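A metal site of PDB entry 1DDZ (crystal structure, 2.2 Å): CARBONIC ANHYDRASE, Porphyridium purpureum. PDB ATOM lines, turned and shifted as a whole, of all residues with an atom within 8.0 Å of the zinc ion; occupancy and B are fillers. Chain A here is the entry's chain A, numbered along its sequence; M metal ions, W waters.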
ATOM      1  N   GLY A  73      -7.221  12.324  16.203  1.00  0.00           N
ATOM      2  CA  GLY A  73      -7.504  13.377  17.159  1.00  0.00           C
ATOM      3  C   GLY A  73      -7.261  12.970  18.592  1.00  0.00           C
ATOM      4  O   GLY A  73      -6.761  11.895  18.884  1.00  0.00           O
ATOM      5  N   CYS A  74      -7.645  13.857  19.500  1.00  0.00           N
ATOM      6  CA  CYS A  74      -7.463  13.650  20.908  1.00  0.00           C
ATOM      7  C   CYS A  74      -8.748  13.171  21.561  1.00  0.00           C
ATOM      8  O   CYS A  74      -9.831  13.571  21.168  1.00  0.00           O
ATOM      9  CB  CYS A  74      -7.056  14.991  21.558  1.00  0.00           C
ATOM     10  SG  CYS A  74      -6.729  14.944  23.323  1.00  0.00           S
ATOM     11  N   ALA A  75      -8.587  12.364  22.608  1.00  0.00           N
ATOM     12  CA  ALA A  75      -9.714  11.828  23.355  1.00  0.00           C
ATOM     13  C   ALA A  75     -10.548  12.863  24.096  1.00  0.00           C
ATOM     14  O   ALA A  75     -11.682  12.576  24.390  1.00  0.00           O
ATOM     15  CB  ALA A  75      -9.248  10.771  24.327  1.00  0.00           C
ATOM     16  N   ASP A  76      -9.985  14.016  24.480  1.00  0.00           N
ATOM     17  CA  ASP A  76     -10.789  15.034  25.179  1.00  0.00           C
ATOM     18  C   ASP A  76     -11.219  16.081  24.207  1.00  0.00           C
ATOM     19  O   ASP A  76     -10.979  17.254  24.437  1.00  0.00           O
ATOM     20  CB  ASP A  76     -10.113  15.716  26.409  1.00  0.00           C
ATOM     21  CG  ASP A  76      -8.600  15.766  26.306  1.00  0.00           C
ATOM     22  OD1 ASP A  76      -7.970  14.937  26.979  1.00  0.00           O
ATOM     23  OD2 ASP A  76      -8.039  16.592  25.521  1.00  0.00           O
ATOM     24  N   SER A  77     -11.905  15.695  23.134  1.00  0.00           N
ATOM     25  CA  SER A  77     -12.327  16.673  22.149  1.00  0.00           C
ATOM     26  C   SER A  77     -13.792  16.969  22.066  1.00  0.00           C
ATOM     27  O   SER A  77     -14.662  16.093  22.009  1.00  0.00           O
ATOM     28  CB  SER A  77     -11.687  16.368  20.767  1.00  0.00           C
ATOM     29  OG  SER A  77     -10.297  16.716  20.889  1.00  0.00           O
ATOM     30  N   ARG A  78     -14.071  18.249  22.186  1.00  0.00           N
ATOM     31  CA  ARG A  78     -15.434  18.742  22.222  1.00  0.00           C
ATOM     32  C   ARG A  78     -16.110  18.896  20.895  1.00  0.00           C
ATOM     33  O   ARG A  78     -17.202  19.438  20.835  1.00  0.00           O
ATOM     34  CB  ARG A  78     -15.529  20.065  23.003  1.00  0.00           C
ATOM     35  CG  ARG A  78     -15.033  19.945  24.433  1.00  0.00           C
ATOM     36  CD  ARG A  78     -14.968  21.285  25.089  1.00  0.00           C
ATOM     37  NE  ARG A  78     -14.932  21.165  26.545  1.00  0.00           N
ATOM     38  CZ  ARG A  78     -14.723  22.177  27.381  1.00  0.00           C
ATOM     39  NH1 ARG A  78     -14.521  23.404  26.894  1.00  0.00           N
ATOM     40  NH2 ARG A  78     -14.762  21.990  28.692  1.00  0.00           N
ATOM     41  N   ASN A  97      -6.858   9.349  20.760  1.00  0.00           N
ATOM     42  CA  ASN A  97      -6.010   8.915  21.866  1.00  0.00           C
ATOM     43  C   ASN A  97      -5.629  10.152  22.657  1.00  0.00           C
ATOM     44  O   ASN A  97      -6.097  11.246  22.348  1.00  0.00           O
ATOM     45  CB  ASN A  97      -4.789   8.140  21.351  1.00  0.00           C
ATOM     46  CG  ASN A  97      -3.829   9.021  20.576  1.00  0.00           C
ATOM     47  OD1 ASN A  97      -3.841  10.253  20.704  1.00  0.00           O
ATOM     48  ND2 ASN A  97      -3.008   8.406  19.747  1.00  0.00           N
ATOM     49  N   ILE A  98      -4.833   9.970  23.712  1.00  0.00           N
ATOM     50  CA  ILE A  98      -4.407  11.082  24.544  1.00  0.00           C
ATOM     51  C   ILE A  98      -3.431  11.976  23.775  1.00  0.00           C
ATOM     52  O   ILE A  98      -2.353  11.526  23.349  1.00  0.00           O
ATOM     53  CB  ILE A  98      -3.727  10.598  25.864  1.00  0.00           C
ATOM     54  CG1 ILE A  98      -4.754   9.883  26.766  1.00  0.00           C
ATOM     55  CG2 ILE A  98      -3.079  11.782  26.611  1.00  0.00           C
ATOM     56  CD1 ILE A  98      -5.877  10.789  27.243  1.00  0.00           C
ATOM     57  N   ALA A  99      -3.825  13.236  23.581  1.00  0.00           N
ATOM     58  CA  ALA A  99      -3.013  14.234  22.898  1.00  0.00           C
ATOM     59  C   ALA A  99      -2.700  13.968  21.437  1.00  0.00           C
ATOM     60  O   ALA A  99      -1.637  14.337  20.954  1.00  0.00           O
ATOM     61  CB  ALA A  99      -1.715  14.494  23.662  1.00  0.00           C
ATOM     62  N   ASN A 100      -3.633  13.312  20.721  1.00  0.00           N
ATOM     63  CA  ASN A 100      -3.487  13.034  19.292  1.00  0.00           C
ATOM     64  C   ASN A 100      -2.078  12.613  18.832  1.00  0.00           C
ATOM     65  O   ASN A 100      -1.540  13.118  17.853  1.00  0.00           O
ATOM     66  CB  ASN A 100      -4.013  14.223  18.433  1.00  0.00           C
ATOM     67  CG  ASN A 100      -3.502  15.600  18.919  1.00  0.00           C
ATOM     68  OD1 ASN A 100      -4.121  16.240  19.768  1.00  0.00           O
ATOM     69  ND2 ASN A 100      -2.394  16.045  18.370  1.00  0.00           N
ATOM     70  N   CYS A 128      -5.238  16.330  14.081  1.00  0.00           N
ATOM     71  CA  CYS A 128      -5.821  17.517  14.664  1.00  0.00           C
ATOM     72  C   CYS A 128      -5.603  17.607  16.149  1.00  0.00           C
ATOM     73  O   CYS A 128      -5.882  16.652  16.873  1.00  0.00           O
ATOM     74  CB  CYS A 128      -7.328  17.573  14.374  1.00  0.00           C
ATOM     75  SG  CYS A 128      -8.190  18.948  15.096  1.00  0.00           S
ATOM     76  N   GLY A 129      -5.083  18.753  16.585  1.00  0.00           N
ATOM     77  CA  GLY A 129      -4.839  18.999  17.989  1.00  0.00           C
ATOM     78  C   GLY A 129      -5.817  20.088  18.374  1.00  0.00           C
ATOM     79  O   GLY A 129      -6.447  20.678  17.487  1.00  0.00           O
ATOM     80  N   HIS A 130      -5.900  20.413  19.654  1.00  0.00           N
ATOM     81  CA  HIS A 130      -6.819  21.453  20.093  1.00  0.00           C
ATOM     82  C   HIS A 130      -6.199  22.219  21.255  1.00  0.00           C
ATOM     83  O   HIS A 130      -5.531  21.653  22.104  1.00  0.00           O
ATOM     84  CB  HIS A 130      -8.160  20.813  20.508  1.00  0.00           C
ATOM     85  CG  HIS A 130      -8.058  19.860  21.661  1.00  0.00           C
ATOM     86  ND1 HIS A 130      -8.744  20.045  22.833  1.00  0.00           N
ATOM     87  CD2 HIS A 130      -7.308  18.740  21.832  1.00  0.00           C
ATOM     88  CE1 HIS A 130      -8.420  19.074  23.679  1.00  0.00           C
ATOM     89  NE2 HIS A 130      -7.543  18.268  23.102  1.00  0.00           N
ATOM     90  N   TYR A 131      -6.413  23.528  21.286  1.00  0.00           N
ATOM     91  CA  TYR A 131      -5.867  24.371  22.341  1.00  0.00           C
ATOM     92  C   TYR A 131      -6.475  23.960  23.666  1.00  0.00           C
ATOM     93  O   TYR A 131      -7.603  23.496  23.702  1.00  0.00           O
ATOM     94  CB  TYR A 131      -6.118  25.854  22.045  1.00  0.00           C
ATOM     95  CG  TYR A 131      -5.378  26.323  20.813  1.00  0.00           C
ATOM     96  CD1 TYR A 131      -6.061  26.897  19.752  1.00  0.00           C
ATOM     97  CD2 TYR A 131      -3.995  26.171  20.702  1.00  0.00           C
ATOM     98  CE1 TYR A 131      -5.391  27.307  18.613  1.00  0.00           C
ATOM     99  CE2 TYR A 131      -3.313  26.587  19.553  1.00  0.00           C
ATOM    100  CZ  TYR A 131      -4.020  27.143  18.520  1.00  0.00           C
ATOM    101  OH  TYR A 131      -3.357  27.547  17.378  1.00  0.00           O
ATOM    102  N   GLY A 132      -5.692  24.060  24.746  1.00  0.00           N
ATOM    103  CA  GLY A 132      -6.172  23.660  26.069  1.00  0.00           C
ATOM    104  C   GLY A 132      -6.140  22.150  26.322  1.00  0.00           C
ATOM    105  O   GLY A 132      -6.577  21.685  27.372  1.00  0.00           O
ATOM    106  N   CYS A 133      -5.572  21.386  25.383  1.00  0.00           N
ATOM    107  CA  CYS A 133      -5.476  19.946  25.502  1.00  0.00           C
ATOM    108  C   CYS A 133      -4.982  19.479  26.876  1.00  0.00           C
ATOM    109  O   CYS A 133      -3.841  19.763  27.240  1.00  0.00           O
ATOM    110  CB  CYS A 133      -4.529  19.420  24.419  1.00  0.00           C
ATOM    111  SG  CYS A 133      -4.332  17.630  24.403  1.00  0.00           S
ATOM    112  N   GLY A 134      -5.833  18.751  27.605  1.00  0.00           N
ATOM    113  CA  GLY A 134      -5.488  18.214  28.918  1.00  0.00           C
ATOM    114  C   GLY A 134      -4.261  17.312  28.879  1.00  0.00           C
ATOM    115  O   GLY A 134      -3.483  17.284  29.835  1.00  0.00           O
ATOM    116  N   GLY A 135      -4.057  16.584  27.792  1.00  0.00           N
ATOM    117  CA  GLY A 135      -2.883  15.726  27.694  1.00  0.00           C
ATOM    118  C   GLY A 135      -1.585  16.524  27.627  1.00  0.00           C
ATOM    119  O   GLY A 135      -0.620  16.246  28.331  1.00  0.00           O
ATOM    120  N   ALA A 136      -1.583  17.548  26.776  1.00  0.00           N
ATOM    121  CA  ALA A 136      -0.415  18.405  26.612  1.00  0.00           C
ATOM    122  C   ALA A 136      -0.142  19.170  27.892  1.00  0.00           C
ATOM    123  O   ALA A 136       0.994  19.339  28.300  1.00  0.00           O
ATOM    124  CB  ALA A 136      -0.661  19.369  25.454  1.00  0.00           C
ATOM    125  N   LYS A 137      -1.216  19.600  28.549  1.00  0.00           N
ATOM    126  CA  LYS A 137      -1.149  20.352  29.791  1.00  0.00           C
ATOM    127  C   LYS A 137      -0.561  19.527  30.928  1.00  0.00           C
ATOM    128  O   LYS A 137       0.311  20.002  31.664  1.00  0.00           O
ATOM    129  CB  LYS A 137      -2.547  20.836  30.134  1.00  0.00           C
ATOM    130  CG  LYS A 137      -2.635  21.862  31.200  1.00  0.00           C
ATOM    131  CD  LYS A 137      -4.068  22.336  31.345  1.00  0.00           C
ATOM    132  CE  LYS A 137      -4.238  23.160  32.591  1.00  0.00           C
ATOM    133  NZ  LYS A 137      -5.583  23.798  32.688  1.00  0.00           N
ATOM    134  N   ILE A 180       1.236  22.688  21.769  1.00  0.00           N
ATOM    135  CA  ILE A 180       0.148  22.004  21.120  1.00  0.00           C
ATOM    136  C   ILE A 180       0.322  22.061  19.611  1.00  0.00           C
ATOM    137  O   ILE A 180       0.250  21.050  18.937  1.00  0.00           O
ATOM    138  CB  ILE A 180      -1.206  22.566  21.594  1.00  0.00           C
ATOM    139  CG1 ILE A 180      -1.432  22.084  23.028  1.00  0.00           C
ATOM    140  CG2 ILE A 180      -2.371  22.118  20.655  1.00  0.00           C
ATOM    141  CD1 ILE A 180      -2.584  22.772  23.752  1.00  0.00           C
ATOM    142  N   PHE A 347     -15.636  11.412  26.835  1.00  0.00           N
ATOM    143  CA  PHE A 347     -14.214  11.237  26.542  1.00  0.00           C
ATOM    144  C   PHE A 347     -14.216  10.041  25.606  1.00  0.00           C
ATOM    145  O   PHE A 347     -14.766   9.007  25.952  1.00  0.00           O
ATOM    146  CB  PHE A 347     -13.517  10.880  27.861  1.00  0.00           C
ATOM    147  CG  PHE A 347     -12.039  11.161  27.874  1.00  0.00           C
ATOM    148  CD1 PHE A 347     -11.555  12.461  27.784  1.00  0.00           C
ATOM    149  CD2 PHE A 347     -11.125  10.105  28.012  1.00  0.00           C
ATOM    150  CE1 PHE A 347     -10.178  12.710  27.839  1.00  0.00           C
ATOM    151  CE2 PHE A 347      -9.741  10.348  28.063  1.00  0.00           C
ATOM    152  CZ  PHE A 347      -9.271  11.648  27.975  1.00  0.00           C
ATOM    153  N   TYR A 369      -6.394   7.824  32.466  1.00  0.00           N
ATOM    154  CA  TYR A 369      -6.704   9.234  32.497  1.00  0.00           C
ATOM    155  C   TYR A 369      -8.193   9.477  32.848  1.00  0.00           C
ATOM    156  O   TYR A 369      -8.505  10.325  33.692  1.00  0.00           O
ATOM    157  CB  TYR A 369      -6.378   9.877  31.158  1.00  0.00           C
ATOM    158  CG  TYR A 369      -6.527  11.386  31.194  1.00  0.00           C
ATOM    159  CD1 TYR A 369      -5.491  12.193  31.654  1.00  0.00           C
ATOM    160  CD2 TYR A 369      -7.704  12.013  30.802  1.00  0.00           C
ATOM    161  CE1 TYR A 369      -5.609  13.564  31.725  1.00  0.00           C
ATOM    162  CE2 TYR A 369      -7.844  13.395  30.871  1.00  0.00           C
ATOM    163  CZ  TYR A 369      -6.793  14.168  31.330  1.00  0.00           C
ATOM    164  OH  TYR A 369      -6.902  15.540  31.412  1.00  0.00           O
HETATM  165 ZN    ZN M   1      -6.585  17.061  24.441  1.00  0.00          ZN
HETATM  166  O   HOH W   1      -5.793  14.464  26.075  1.00  0.00           O
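The side-chain sulfur of Cys 133 sits close to the backbone NH of Gly 135, 3.6 Å away.
SG of Cys 133 lies close to N of Ala 136.
The side-chain sulfur (SG) of Cys 74 lies close to the backbone NH (N) of Ala 99, 3.4 Å away.
OG of Ser 77 lies within hydrogen-bond range of O of Cys 74 (3.2 Å).
Gly 134 touches the zinc ion (N to ZN, 3.7 Å).
The nearest printed residue that does not touch the zinc ion is Gly 135 (4.2 Å).
OD2 of Asp 76 is bound to the zinc ion (1.9 Å).
NE2 of His 130 is bound to the zinc ion (2.0 Å).
The side-chain sulfur (SG) of Cys 133 binds the zinc ion, 2.3 Å away.
The side-chain sulfur (SG) of Cys 74 binds the zinc ion.
Water W1 lies within hydrogen-bond range of the side-chain carboxylate (OD1) of Asp 76 (2.4 Å), the backbone NH (N) of Gly 135 (3.2 Å) and the backbone NH (N) of Ala 99 (3.4 Å).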
